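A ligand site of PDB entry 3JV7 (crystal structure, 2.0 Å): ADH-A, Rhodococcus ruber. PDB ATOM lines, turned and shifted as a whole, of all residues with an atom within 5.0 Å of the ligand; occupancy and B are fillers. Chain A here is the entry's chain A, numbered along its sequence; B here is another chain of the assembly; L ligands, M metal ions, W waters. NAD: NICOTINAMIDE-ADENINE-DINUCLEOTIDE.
The side-chain carboxylate (OD2) of Asp 203 sits at hydrogen-bond distance from an oxygen (O2B) of the ligand (2.6 Å). An oxygen (O7N) of the ligand lies within hydrogen-bond range of the backbone NH (N) of Trp 295, 2.7 Å away. OG of Ser 40 lies within hydrogen-bond range of O2D of the ligand, at 2.7 Å. The side-chain hydroxyl of Ser 223 is in hydrogen-bond range of a nitrogen (N1A) of the ligand (2.7 Å). The backbone NH (N) of His 39 sits at hydrogen-bond distance from an oxygen (O1N) of the ligand, 3.0 Å away. A ring nitrogen (ND1) of His 39 lies within hydrogen-bond range of an oxygen (O1A) of the ligand, 2.8 Å away. An oxygen (O1N) of the ligand is in salt-bridge range of the guanidinium group of Arg 340, at 2.8 Å. O2N of the ligand is in hydrogen-bond range of N of Leu 183. N of Ile 271 lies within hydrogen-bond range of O3D of the ligand, at 3.0 Å. An oxygen (O2A) of the ligand lies within hydrogen-bond range of the backbone NH (N) of Gly 182 (3.0 Å). O of Pro 293 lies within hydrogen-bond range of N7N of the ligand (3.1 Å). O of Val 269 lies within hydrogen-bond range of N7N of the ligand (3.1 Å). The guanidinium group (NH1) of Arg 208 lies within hydrogen-bond range of an oxygen (O3B) of the ligand, 3.2 Å away. O3B of the ligand is in hydrogen-bond range of O of Val 180, 3.5 Å away.
The backbone NH (N) of Ser 223 lies within hydrogen-bond range of the backbone carbonyl oxygen (O) of Asp 203. The backbone NH of Val 180 sits at hydrogen-bond distance from the side-chain carboxylate of Asp 203 (2.8 Å). OD2 of Asp 203 lies within hydrogen-bond range of N of Asp 205 (2.9 Å). The side-chain sulfur (SG) of Cys 38 sits close to the backbone NH (N) of Ser 40, at 3.4 Å. The guanidinium group of Arg 340 sits close to the side-chain sulfur of Cys 38 (3.5 Å). O of Leu 37 sits close to NE of Arg 340. The backbone NH (N) of Phe 246 sits at hydrogen-bond distance from the backbone carbonyl oxygen (O) of Ile 178, 2.8 Å away. The side-chain carboxylate (OD1) of Asp 153 sits at hydrogen-bond distance from the side-chain hydroxyl (OG1) of Thr 157.
SG of Cys 38 touches C6N of the ligand, at 3.7 Å. Asp 153 touches the ligand. Thr 157 touches the ligand (CG2 to C4N, 3.5 Å). Ile 178 touches the ligand (CG2 to C2A, 3.98 Å). Gly 179 touches the ligand (CA to O4B, 3.8 Å). Gly 181 touches the ligand (CA to O5B, 3.3 Å). N of Leu 204 touches N3A of the ligand, at 3.5 Å. Phe 246 touches the ligand. Val 247 touches the ligand (CG2 to C4A, 3.3 Å). CG2 of Thr 252 touches N1A of the ligand (3.5 Å). Gly 270 touches the ligand. Tyr 294 touches the ligand (CA to O7N, 3.5 Å). Leu 332 touches the ligand. Phe 281 of chain B touches the ligand. Hydrophobic or aromatic side chains within 4 Å of the ligand: His 39, Ile 178, Leu 183, Leu 204, Val 247, Val 269, Ile 271, Tyr 294, Leu 332 and Phe 281 of chain B. Of the 33 residues printed, 27 come within 4 Å of the ligand. The nearest printed residue that does not touch the ligand is Val 202 (4.1 Å).
Water W5 lies within hydrogen-bond range of O1A of the ligand (2.6 Å) and O of Leu 332 (2.8 Å). Water W3 lies within hydrogen-bond range of O2A of the ligand (2.7 Å), O of Gly 339 (2.7 Å) and NH1 of Arg 340 (3.0 Å). Water W1 lies within hydrogen-bond range of an oxygen (O2D) of the ligand (2.9 Å) and the backbone carbonyl oxygen (O) of Ile 271 (3.1 Å). Water W4 lies within hydrogen-bond range of an oxygen (O2A) of the ligand, the backbone carbonyl oxygen (O) of Gly 339 and the guanidinium group (NH1) of Arg 208. Water W9 bridges the backbone carbonyl oxygen (O) of Phe 246 and an oxygen (O4B) of the ligand. Water W8 lies within hydrogen-bond range of OG of Ser 251, N6A of the ligand and OG of Ser 223.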
ATOM      1  N   LEU A  37       3.229 -10.273  -9.158  1.00  0.00           N
ATOM      2  CA  LEU A  37       2.949  -9.151 -10.061  1.00  0.00           C
ATOM      3  C   LEU A  37       1.915  -8.235  -9.434  1.00  0.00           C
ATOM      4  O   LEU A  37       0.890  -8.699  -8.945  1.00  0.00           O
ATOM      5  CB  LEU A  37       2.402  -9.644 -11.400  1.00  0.00           C
ATOM      6  CG  LEU A  37       3.392 -10.301 -12.363  1.00  0.00           C
ATOM      7  CD1 LEU A  37       3.713 -11.746 -11.942  1.00  0.00           C
ATOM      8  CD2 LEU A  37       2.847 -10.263 -13.787  1.00  0.00           C
ATOM      9  N   CYS A  38       2.194  -6.935  -9.443  1.00  0.00           N
ATOM     10  CA  CYS A  38       1.293  -5.948  -8.881  1.00  0.00           C
ATOM     11  C   CYS A  38       0.854  -4.982  -9.967  1.00  0.00           C
ATOM     12  O   CYS A  38       1.624  -4.644 -10.857  1.00  0.00           O
ATOM     13  CB  CYS A  38       1.974  -5.167  -7.751  1.00  0.00           C
ATOM     14  SG  CYS A  38       0.915  -3.917  -7.012  1.00  0.00           S
ATOM     15  N   HIS A  39      -0.388  -4.512  -9.897  1.00  0.00           N
ATOM     16  CA  HIS A  39      -0.856  -3.556 -10.896  1.00  0.00           C
ATOM     17  C   HIS A  39      -0.038  -2.254 -10.840  1.00  0.00           C
ATOM     18  O   HIS A  39      -0.039  -1.487 -11.814  1.00  0.00           O
ATOM     19  CB  HIS A  39      -2.354  -3.282 -10.722  1.00  0.00           C
ATOM     20  CG  HIS A  39      -3.002  -2.736 -11.966  1.00  0.00           C
ATOM     21  ND1 HIS A  39      -3.905  -3.465 -12.708  1.00  0.00           N
ATOM     22  CD2 HIS A  39      -2.867  -1.554 -12.599  1.00  0.00           C
ATOM     23  CE1 HIS A  39      -4.309  -2.748 -13.735  1.00  0.00           C
ATOM     24  NE2 HIS A  39      -3.692  -1.585 -13.703  1.00  0.00           N
ATOM     25  N   SER A  40       0.645  -1.989  -9.745  1.00  0.00           N
ATOM     26  CA  SER A  40       1.507  -0.802  -9.720  1.00  0.00           C
ATOM     27  C   SER A  40       2.617  -0.912 -10.765  1.00  0.00           C
ATOM     28  O   SER A  40       3.128   0.099 -11.260  1.00  0.00           O
ATOM     29  CB  SER A  40       2.097  -0.531  -8.332  1.00  0.00           C
ATOM     30  OG  SER A  40       1.069  -0.149  -7.421  1.00  0.00           O
ATOM     31  N   ASP A 153       2.461  -7.353  -0.203  1.00  0.00           N
ATOM     32  CA  ASP A 153       1.912  -6.118  -0.765  1.00  0.00           C
ATOM     33  C   ASP A 153       0.396  -6.232  -0.904  1.00  0.00           C
ATOM     34  O   ASP A 153      -0.352  -5.439  -0.325  1.00  0.00           O
ATOM     35  CB  ASP A 153       2.594  -5.834  -2.105  1.00  0.00           C
ATOM     36  CG  ASP A 153       2.126  -4.547  -2.763  1.00  0.00           C
ATOM     37  OD1 ASP A 153       1.317  -3.785  -2.165  1.00  0.00           O
ATOM     38  OD2 ASP A 153       2.569  -4.318  -3.909  1.00  0.00           O
ATOM     39  N   THR A 157      -0.554  -4.018   2.065  1.00  0.00           N
ATOM     40  CA  THR A 157      -1.141  -2.722   1.759  1.00  0.00           C
ATOM     41  C   THR A 157      -2.587  -2.542   2.258  1.00  0.00           C
ATOM     42  O   THR A 157      -2.871  -1.580   2.982  1.00  0.00           O
ATOM     43  CB  THR A 157      -0.943  -2.363   0.278  1.00  0.00           C
ATOM     44  OG1 THR A 157       0.473  -2.301   0.019  1.00  0.00           O
ATOM     45  CG2 THR A 157      -1.580  -1.019  -0.046  1.00  0.00           C
ATOM     46  N   ILE A 178     -13.752  -1.573  -2.871  1.00  0.00           N
ATOM     47  CA  ILE A 178     -13.939  -1.325  -4.289  1.00  0.00           C
ATOM     48  C   ILE A 178     -12.716  -1.846  -5.030  1.00  0.00           C
ATOM     49  O   ILE A 178     -11.585  -1.397  -4.783  1.00  0.00           O
ATOM     50  CB  ILE A 178     -14.119   0.178  -4.603  1.00  0.00           C
ATOM     51  CG1 ILE A 178     -15.173   0.808  -3.690  1.00  0.00           C
ATOM     52  CG2 ILE A 178     -14.496   0.350  -6.077  1.00  0.00           C
ATOM     53  CD1 ILE A 178     -15.480   2.301  -4.054  1.00  0.00           C
ATOM     54  N   GLY A 179     -12.939  -2.814  -5.908  1.00  0.00           N
ATOM     55  CA  GLY A 179     -11.880  -3.449  -6.659  1.00  0.00           C
ATOM     56  C   GLY A 179     -11.526  -4.771  -6.020  1.00  0.00           C
ATOM     57  O   GLY A 179     -10.846  -4.806  -4.982  1.00  0.00           O
ATOM     58  N   VAL A 180     -12.006  -5.862  -6.609  1.00  0.00           N
ATOM     59  CA  VAL A 180     -11.733  -7.196  -6.057  1.00  0.00           C
ATOM     60  C   VAL A 180     -10.668  -7.896  -6.896  1.00  0.00           C
ATOM     61  O   VAL A 180     -10.935  -8.919  -7.548  1.00  0.00           O
ATOM     62  CB  VAL A 180     -13.016  -8.050  -5.981  1.00  0.00           C
ATOM     63  CG1 VAL A 180     -12.743  -9.386  -5.291  1.00  0.00           C
ATOM     64  CG2 VAL A 180     -14.119  -7.282  -5.251  1.00  0.00           C
ATOM     65  N   GLY A 181      -9.459  -7.334  -6.875  1.00  0.00           N
ATOM     66  CA  GLY A 181      -8.309  -7.868  -7.596  1.00  0.00           C
ATOM     67  C   GLY A 181      -7.307  -8.485  -6.640  1.00  0.00           C
ATOM     68  O   GLY A 181      -7.687  -9.076  -5.633  1.00  0.00           O
ATOM     69  N   GLY A 182      -6.020  -8.359  -6.949  1.00  0.00           N
ATOM     70  CA  GLY A 182      -4.986  -8.832  -6.056  1.00  0.00           C
ATOM     71  C   GLY A 182      -5.122  -8.319  -4.633  1.00  0.00           C
ATOM     72  O   GLY A 182      -5.210  -9.126  -3.691  1.00  0.00           O
ATOM     73  N   LEU A 183      -5.138  -6.993  -4.459  1.00  0.00           N
ATOM     74  CA  LEU A 183      -5.285  -6.383  -3.135  1.00  0.00           C
ATOM     75  C   LEU A 183      -6.688  -6.588  -2.561  1.00  0.00           C
ATOM     76  O   LEU A 183      -6.846  -6.957  -1.410  1.00  0.00           O
ATOM     77  CB  LEU A 183      -5.012  -4.858  -3.186  1.00  0.00           C
ATOM     78  CG  LEU A 183      -3.568  -4.371  -2.943  1.00  0.00           C
ATOM     79  CD1 LEU A 183      -2.657  -4.819  -4.080  1.00  0.00           C
ATOM     80  CD2 LEU A 183      -3.511  -2.859  -2.788  1.00  0.00           C
ATOM     81  N   GLY A 184      -7.708  -6.335  -3.383  1.00  0.00           N
ATOM     82  CA  GLY A 184      -9.069  -6.314  -2.897  1.00  0.00           C
ATOM     83  C   GLY A 184      -9.543  -7.649  -2.345  1.00  0.00           C
ATOM     84  O   GLY A 184     -10.235  -7.695  -1.333  1.00  0.00           O
ATOM     85  N   VAL A 202     -17.300  -4.316  -4.382  1.00  0.00           N
ATOM     86  CA  VAL A 202     -17.716  -3.615  -5.592  1.00  0.00           C
ATOM     87  C   VAL A 202     -16.699  -3.903  -6.707  1.00  0.00           C
ATOM     88  O   VAL A 202     -15.489  -3.807  -6.496  1.00  0.00           O
ATOM     89  CB  VAL A 202     -17.810  -2.100  -5.356  1.00  0.00           C
ATOM     90  CG1 VAL A 202     -18.296  -1.386  -6.640  1.00  0.00           C
ATOM     91  CG2 VAL A 202     -18.754  -1.773  -4.195  1.00  0.00           C
ATOM     92  N   ASP A 203     -17.188  -4.277  -7.886  1.00  0.00           N
ATOM     93  CA  ASP A 203     -16.279  -4.498  -9.028  1.00  0.00           C
ATOM     94  C   ASP A 203     -17.007  -4.349 -10.361  1.00  0.00           C
ATOM     95  O   ASP A 203     -18.233  -4.453 -10.431  1.00  0.00           O
ATOM     96  CB  ASP A 203     -15.600  -5.880  -8.916  1.00  0.00           C
ATOM     97  CG  ASP A 203     -14.283  -5.975  -9.700  1.00  0.00           C
ATOM     98  OD1 ASP A 203     -13.216  -6.154  -9.073  1.00  0.00           O
ATOM     99  OD2 ASP A 203     -14.311  -5.865 -10.942  1.00  0.00           O
ATOM    100  N   LEU A 204     -16.254  -4.092 -11.424  1.00  0.00           N
ATOM    101  CA  LEU A 204     -16.878  -3.985 -12.747  1.00  0.00           C
ATOM    102  C   LEU A 204     -17.192  -5.370 -13.289  1.00  0.00           C
ATOM    103  O   LEU A 204     -18.054  -5.518 -14.150  1.00  0.00           O
ATOM    104  CB  LEU A 204     -15.934  -3.291 -13.735  1.00  0.00           C
ATOM    105  CG  LEU A 204     -15.685  -1.785 -13.643  1.00  0.00           C
ATOM    106  CD1 LEU A 204     -14.561  -1.386 -14.591  1.00  0.00           C
ATOM    107  CD2 LEU A 204     -16.943  -1.020 -13.977  1.00  0.00           C
ATOM    108  N   ASP A 205     -16.470  -6.374 -12.799  1.00  0.00           N
ATOM    109  CA  ASP A 205     -16.508  -7.697 -13.423  1.00  0.00           C
ATOM    110  C   ASP A 205     -17.334  -8.672 -12.590  1.00  0.00           C
ATOM    111  O   ASP A 205     -17.038  -8.900 -11.413  1.00  0.00           O
ATOM    112  CB  ASP A 205     -15.064  -8.221 -13.614  1.00  0.00           C
ATOM    113  CG  ASP A 205     -15.007  -9.558 -14.361  1.00  0.00           C
ATOM    114  OD1 ASP A 205     -15.987 -10.326 -14.323  1.00  0.00           O
ATOM    115  OD2 ASP A 205     -13.958  -9.842 -14.975  1.00  0.00           O
ATOM    116  N   ARG A 208     -15.572 -11.253 -10.748  1.00  0.00           N
ATOM    117  CA  ARG A 208     -14.892 -10.741  -9.559  1.00  0.00           C
ATOM    118  C   ARG A 208     -15.881 -10.549  -8.407  1.00  0.00           C
ATOM    119  O   ARG A 208     -15.497 -10.678  -7.238  1.00  0.00           O
ATOM    120  CB  ARG A 208     -14.135  -9.436  -9.877  1.00  0.00           C
ATOM    121  CG  ARG A 208     -13.062  -9.582 -10.962  1.00  0.00           C
ATOM    122  CD  ARG A 208     -12.059 -10.683 -10.630  1.00  0.00           C
ATOM    123  NE  ARG A 208     -11.153 -10.971 -11.737  1.00  0.00           N
ATOM    124  CZ  ARG A 208      -9.921 -10.473 -11.865  1.00  0.00           C
ATOM    125  NH1 ARG A 208      -9.429  -9.651 -10.935  1.00  0.00           N
ATOM    126  NH2 ARG A 208      -9.186 -10.799 -12.914  1.00  0.00           N
ATOM    127  N   SER A 223     -20.055  -2.185 -10.081  1.00  0.00           N
ATOM    128  CA  SER A 223     -19.516  -0.838 -10.000  1.00  0.00           C
ATOM    129  C   SER A 223     -20.129   0.067 -11.071  1.00  0.00           C
ATOM    130  O   SER A 223     -20.806  -0.421 -11.974  1.00  0.00           O
ATOM    131  CB  SER A 223     -17.992  -0.886 -10.200  1.00  0.00           C
ATOM    132  OG  SER A 223     -17.384   0.352  -9.849  1.00  0.00           O
ATOM    133  N   PHE A 246      -9.630   0.294  -3.842  1.00  0.00           N
ATOM    134  CA  PHE A 246      -8.394  -0.244  -4.387  1.00  0.00           C
ATOM    135  C   PHE A 246      -8.323  -0.022  -5.891  1.00  0.00           C
ATOM    136  O   PHE A 246      -7.462  -0.589  -6.549  1.00  0.00           O
ATOM    137  CB  PHE A 246      -8.239  -1.737  -4.047  1.00  0.00           C
ATOM    138  CG  PHE A 246      -8.214  -2.012  -2.574  1.00  0.00           C
ATOM    139  CD1 PHE A 246      -7.052  -1.795  -1.827  1.00  0.00           C
ATOM    140  CD2 PHE A 246      -9.345  -2.482  -1.917  1.00  0.00           C
ATOM    141  CE1 PHE A 246      -7.025  -2.033  -0.467  1.00  0.00           C
ATOM    142  CE2 PHE A 246      -9.330  -2.718  -0.551  1.00  0.00           C
ATOM    143  CZ  PHE A 246      -8.160  -2.494   0.179  1.00  0.00           C
ATOM    144  N   VAL A 247      -9.235   0.791  -6.429  1.00  0.00           N
ATOM    145  CA  VAL A 247      -9.178   1.204  -7.841  1.00  0.00           C
ATOM    146  C   VAL A 247      -8.661   2.637  -7.938  1.00  0.00           C
ATOM    147  O   VAL A 247      -7.681   2.910  -8.626  1.00  0.00           O
ATOM    148  CB  VAL A 247     -10.544   1.148  -8.524  1.00  0.00           C
ATOM    149  CG1 VAL A 247     -10.423   1.638  -9.996  1.00  0.00           C
ATOM    150  CG2 VAL A 247     -11.126  -0.270  -8.464  1.00  0.00           C
ATOM    151  N   SER A 251     -14.147   7.996 -10.755  1.00  0.00           N
ATOM    152  CA  SER A 251     -15.509   7.477 -10.591  1.00  0.00           C
ATOM    153  C   SER A 251     -15.679   6.684  -9.290  1.00  0.00           C
ATOM    154  O   SER A 251     -16.699   6.824  -8.619  1.00  0.00           O
ATOM    155  CB  SER A 251     -15.902   6.609 -11.790  1.00  0.00           C
ATOM    156  OG  SER A 251     -15.002   5.516 -11.939  1.00  0.00           O
ATOM    157  N   THR A 252     -14.704   5.857  -8.935  1.00  0.00           N
ATOM    158  CA  THR A 252     -14.801   5.072  -7.713  1.00  0.00           C
ATOM    159  C   THR A 252     -14.661   5.938  -6.470  1.00  0.00           C
ATOM    160  O   THR A 252     -15.299   5.690  -5.454  1.00  0.00           O
ATOM    161  CB  THR A 252     -13.781   3.907  -7.658  1.00  0.00           C
ATOM    162  OG1 THR A 252     -12.439   4.437  -7.760  1.00  0.00           O
ATOM    163  CG2 THR A 252     -14.044   2.916  -8.816  1.00  0.00           C
ATOM    164  N   VAL A 269      -6.606   3.856  -2.101  1.00  0.00           N
ATOM    165  CA  VAL A 269      -5.459   2.971  -2.147  1.00  0.00           C
ATOM    166  C   VAL A 269      -4.997   2.788  -3.573  1.00  0.00           C
ATOM    167  O   VAL A 269      -3.806   2.847  -3.857  1.00  0.00           O
ATOM    168  CB  VAL A 269      -5.773   1.609  -1.484  1.00  0.00           C
ATOM    169  CG1 VAL A 269      -4.520   0.762  -1.376  1.00  0.00           C
ATOM    170  CG2 VAL A 269      -6.379   1.818  -0.092  1.00  0.00           C
ATOM    171  N   GLY A 270      -5.951   2.571  -4.478  1.00  0.00           N
ATOM    172  CA  GLY A 270      -5.649   2.407  -5.890  1.00  0.00           C
ATOM    173  C   GLY A 270      -5.104   3.683  -6.487  1.00  0.00           C
ATOM    174  O   GLY A 270      -5.428   4.779  -6.037  1.00  0.00           O
ATOM    175  N   ILE A 271      -4.283   3.536  -7.529  1.00  0.00           N
ATOM    176  CA  ILE A 271      -3.546   4.646  -8.105  1.00  0.00           C
ATOM    177  C   ILE A 271      -3.955   4.931  -9.556  1.00  0.00           C
ATOM    178  O   ILE A 271      -3.712   4.107 -10.447  1.00  0.00           O
ATOM    179  CB  ILE A 271      -2.040   4.379  -8.054  1.00  0.00           C
ATOM    180  CG1 ILE A 271      -1.593   4.179  -6.591  1.00  0.00           C
ATOM    181  CG2 ILE A 271      -1.275   5.515  -8.723  1.00  0.00           C
ATOM    182  CD1 ILE A 271      -0.174   3.654  -6.448  1.00  0.00           C
ATOM    183  N   PRO A 293      -2.999   5.950   1.637  1.00  0.00           N
ATOM    184  CA  PRO A 293      -1.944   5.292   2.419  1.00  0.00           C
ATOM    185  C   PRO A 293      -0.894   4.675   1.509  1.00  0.00           C
ATOM    186  O   PRO A 293      -1.151   4.511   0.311  1.00  0.00           O
ATOM    187  CB  PRO A 293      -2.710   4.202   3.162  1.00  0.00           C
ATOM    188  CG  PRO A 293      -3.827   3.803   2.167  1.00  0.00           C
ATOM    189  CD  PRO A 293      -4.089   5.024   1.295  1.00  0.00           C
ATOM    190  N   TYR A 294       0.271   4.348   2.051  1.00  0.00           N
ATOM    191  CA  TYR A 294       1.349   3.748   1.263  1.00  0.00           C
ATOM    192  C   TYR A 294       1.855   2.444   1.875  1.00  0.00           C
ATOM    193  O   TYR A 294       2.378   2.440   2.989  1.00  0.00           O
ATOM    194  CB  TYR A 294       2.490   4.734   1.119  1.00  0.00           C
ATOM    195  CG  TYR A 294       3.738   4.180   0.437  1.00  0.00           C
ATOM    196  CD1 TYR A 294       3.668   3.613  -0.823  1.00  0.00           C
ATOM    197  CD2 TYR A 294       4.985   4.284   1.047  1.00  0.00           C
ATOM    198  CE1 TYR A 294       4.808   3.136  -1.460  1.00  0.00           C
ATOM    199  CE2 TYR A 294       6.134   3.807   0.425  1.00  0.00           C
ATOM    200  CZ  TYR A 294       6.043   3.232  -0.824  1.00  0.00           C
ATOM    201  OH  TYR A 294       7.179   2.768  -1.459  1.00  0.00           O
ATOM    202  N   TRP A 295       1.672   1.339   1.165  1.00  0.00           N
ATOM    203  CA  TRP A 295       2.258   0.067   1.582  1.00  0.00           C
ATOM    204  C   TRP A 295       1.932  -0.233   3.046  1.00  0.00           C
ATOM    205  O   TRP A 295       0.778  -0.127   3.448  1.00  0.00           O
ATOM    206  CB  TRP A 295       3.774   0.046   1.295  1.00  0.00           C
ATOM    207  CG  TRP A 295       4.246  -1.249   0.673  1.00  0.00           C
ATOM    208  CD1 TRP A 295       3.725  -2.486   0.891  1.00  0.00           C
ATOM    209  CD2 TRP A 295       5.329  -1.412  -0.254  1.00  0.00           C
ATOM    210  NE1 TRP A 295       4.408  -3.431   0.150  1.00  0.00           N
ATOM    211  CE2 TRP A 295       5.399  -2.801  -0.563  1.00  0.00           C
ATOM    212  CE3 TRP A 295       6.236  -0.543  -0.856  1.00  0.00           C
ATOM    213  CZ2 TRP A 295       6.353  -3.328  -1.441  1.00  0.00           C
ATOM    214  CZ3 TRP A 295       7.193  -1.067  -1.742  1.00  0.00           C
ATOM    215  CH2 TRP A 295       7.235  -2.449  -2.016  1.00  0.00           C
ATOM    216  N   LEU A 332      -2.271  -9.367 -16.776  1.00  0.00           N
ATOM    217  CA  LEU A 332      -2.640  -8.400 -15.745  1.00  0.00           C
ATOM    218  C   LEU A 332      -3.278  -7.161 -16.370  1.00  0.00           C
ATOM    219  O   LEU A 332      -4.305  -6.667 -15.905  1.00  0.00           O
ATOM    220  CB  LEU A 332      -1.413  -8.003 -14.908  1.00  0.00           C
ATOM    221  CG  LEU A 332      -1.717  -7.185 -13.644  1.00  0.00           C
ATOM    222  CD1 LEU A 332      -2.693  -7.916 -12.717  1.00  0.00           C
ATOM    223  CD2 LEU A 332      -0.431  -6.854 -12.917  1.00  0.00           C
ATOM    224  N   GLY A 339      -7.092 -12.953  -9.232  1.00  0.00           N
ATOM    225  CA  GLY A 339      -6.351 -12.862  -7.985  1.00  0.00           C
ATOM    226  C   GLY A 339      -4.982 -12.288  -8.278  1.00  0.00           C
ATOM    227  O   GLY A 339      -4.871 -11.284  -8.971  1.00  0.00           O
ATOM    228  N   ARG A 340      -3.934 -12.972  -7.818  1.00  0.00           N
ATOM    229  CA  ARG A 340      -2.554 -12.523  -7.987  1.00  0.00           C
ATOM    230  C   ARG A 340      -1.750 -13.413  -8.929  1.00  0.00           C
ATOM    231  O   ARG A 340      -1.741 -14.640  -8.786  1.00  0.00           O
ATOM    232  CB  ARG A 340      -1.852 -12.494  -6.640  1.00  0.00           C
ATOM    233  CG  ARG A 340      -1.677 -11.114  -6.037  1.00  0.00           C
ATOM    234  CD  ARG A 340      -0.616 -10.348  -6.787  1.00  0.00           C
ATOM    235  NE  ARG A 340      -0.183  -9.155  -6.047  1.00  0.00           N
ATOM    236  CZ  ARG A 340      -0.657  -7.930  -6.256  1.00  0.00           C
ATOM    237  NH1 ARG A 340      -1.599  -7.702  -7.166  1.00  0.00           N
ATOM    238  NH2 ARG A 340      -0.187  -6.918  -5.537  1.00  0.00           N
ATOM    239  N   PHE B 281      -2.876  10.627  -5.159  1.00  0.00           N
ATOM    240  CA  PHE B 281      -1.435  10.360  -5.276  1.00  0.00           C
ATOM    241  C   PHE B 281      -0.754  11.435  -6.097  1.00  0.00           C
ATOM    242  O   PHE B 281      -1.315  11.923  -7.066  1.00  0.00           O
ATOM    243  CB  PHE B 281      -1.184   8.960  -5.851  1.00  0.00           C
ATOM    244  CG  PHE B 281      -1.542   7.857  -4.902  1.00  0.00           C
ATOM    245  CD1 PHE B 281      -2.818   7.314  -4.902  1.00  0.00           C
ATOM    246  CD2 PHE B 281      -0.606   7.391  -3.983  1.00  0.00           C
ATOM    247  CE1 PHE B 281      -3.162   6.308  -4.006  1.00  0.00           C
ATOM    248  CE2 PHE B 281      -0.929   6.378  -3.092  1.00  0.00           C
ATOM    249  CZ  PHE B 281      -2.217   5.832  -3.097  1.00  0.00           C
HETATM  250  PA  NAD L   1      -5.502  -5.839 -10.064  1.00  0.00           P
HETATM  251  O1A NAD L   1      -5.227  -5.591 -11.500  1.00  0.00           O
HETATM  252  O2A NAD L   1      -5.062  -7.138  -9.516  1.00  0.00           O
HETATM  253  O5B NAD L   1      -7.072  -5.763  -9.806  1.00  0.00           O
HETATM  254  C5B NAD L   1      -7.877  -4.733 -10.336  1.00  0.00           C
HETATM  255  C4B NAD L   1      -9.326  -5.060  -9.974  1.00  0.00           C
HETATM  256  O4B NAD L   1     -10.029  -3.839  -9.956  1.00  0.00           O
HETATM  257  C3B NAD L   1     -10.012  -5.949 -11.016  1.00  0.00           C
HETATM  258  O3B NAD L   1     -10.860  -6.881 -10.374  1.00  0.00           O
HETATM  259  C2B NAD L   1     -10.880  -4.965 -11.787  1.00  0.00           C
HETATM  260  O2B NAD L   1     -12.066  -5.530 -12.247  1.00  0.00           O
HETATM  261  C1B NAD L   1     -11.202  -3.960 -10.710  1.00  0.00           C
HETATM  262  N9A NAD L   1     -11.618  -2.650 -11.231  1.00  0.00           N
HETATM  263  C8A NAD L   1     -10.981  -1.897 -12.193  1.00  0.00           C
HETATM  264  N7A NAD L   1     -11.694  -0.772 -12.372  1.00  0.00           N
HETATM  265  C5A NAD L   1     -12.767  -0.786 -11.536  1.00  0.00           C
HETATM  266  C6A NAD L   1     -13.784   0.122 -11.330  1.00  0.00           C
HETATM  267  N6A NAD L   1     -13.891   1.178 -12.129  1.00  0.00           N
HETATM  268  N1A NAD L   1     -14.749  -0.155 -10.383  1.00  0.00           N
HETATM  269  C2A NAD L   1     -14.696  -1.334  -9.673  1.00  0.00           C
HETATM  270  N3A NAD L   1     -13.683  -2.234  -9.889  1.00  0.00           N
HETATM  271  C4A NAD L   1     -12.727  -1.962 -10.820  1.00  0.00           C
HETATM  272  O3  NAD L   1      -4.841  -4.599  -9.249  1.00  0.00           O
HETATM  273  PN  NAD L   1      -4.024  -4.741  -7.873  1.00  0.00           P
HETATM  274  O1N NAD L   1      -2.705  -5.350  -8.161  1.00  0.00           O
HETATM  275  O2N NAD L   1      -4.899  -5.322  -6.836  1.00  0.00           O
HETATM  276  O5D NAD L   1      -3.826  -3.176  -7.577  1.00  0.00           O
HETATM  277  C5D NAD L   1      -4.960  -2.354  -7.407  1.00  0.00           C
HETATM  278  C4D NAD L   1      -4.517  -0.895  -7.288  1.00  0.00           C
HETATM  279  O4D NAD L   1      -3.815  -0.722  -6.065  1.00  0.00           O
HETATM  280  C3D NAD L   1      -3.549  -0.460  -8.388  1.00  0.00           C
HETATM  281  O3D NAD L   1      -3.896   0.853  -8.796  1.00  0.00           O
HETATM  282  C2D NAD L   1      -2.211  -0.408  -7.696  1.00  0.00           C
HETATM  283  O2D NAD L   1      -1.397   0.576  -8.267  1.00  0.00           O
HETATM  284  C1D NAD L   1      -2.652   0.047  -6.307  1.00  0.00           C
HETATM  285  N1N NAD L   1      -1.705  -0.218  -5.223  1.00  0.00           N
HETATM  286  C2N NAD L   1      -1.463   0.790  -4.322  1.00  0.00           C
HETATM  287  C3N NAD L   1      -0.607   0.566  -3.255  1.00  0.00           C
HETATM  288  C7N NAD L   1      -0.371   1.649  -2.240  1.00  0.00           C
HETATM  289  O7N NAD L   1       0.651   1.483  -1.307  1.00  0.00           O
HETATM  290  N7N NAD L   1      -1.156   2.716  -2.231  1.00  0.00           N
HETATM  291  C4N NAD L   1      -0.005  -0.691  -3.102  1.00  0.00           C
HETATM  292  C5N NAD L   1      -0.263  -1.709  -4.013  1.00  0.00           C
HETATM  293  C6N NAD L   1      -1.128  -1.459  -5.075  1.00  0.00           C
HETATM  294 ZN    ZN M   1       2.447  -3.162  -5.453  1.00  0.00          ZN
HETATM  295  O   HOH W   1      -2.056   1.508 -10.906  1.00  0.00           O
HETATM  296  O   HOH W   2      -7.502  -1.398 -10.249  1.00  0.00           O
HETATM  297  O   HOH W   3      -3.207  -9.111  -9.222  1.00  0.00           O
HETATM  298  O   HOH W   4      -6.470  -9.437 -10.594  1.00  0.00           O
HETATM  299  O   HOH W   5      -6.061  -6.797 -13.695  1.00  0.00           O
HETATM  300  O   HOH W   6     -12.668   2.571 -14.366  1.00  0.00           O
HETATM  301  O   HOH W   7      -7.514  -5.261  -6.098  1.00  0.00           O
HETATM  302  O   HOH W   8     -16.368   3.210 -11.572  1.00  0.00           O
HETATM  303  O   HOH W   9      -8.568  -2.867  -7.435  1.00  0.00           O
HETATM  304  O   HOH W  10      -6.396   1.170 -10.083  1.00  0.00           O
HETATM  305  O   HOH W  11     -12.372  -5.853 -15.077  1.00  0.00           O
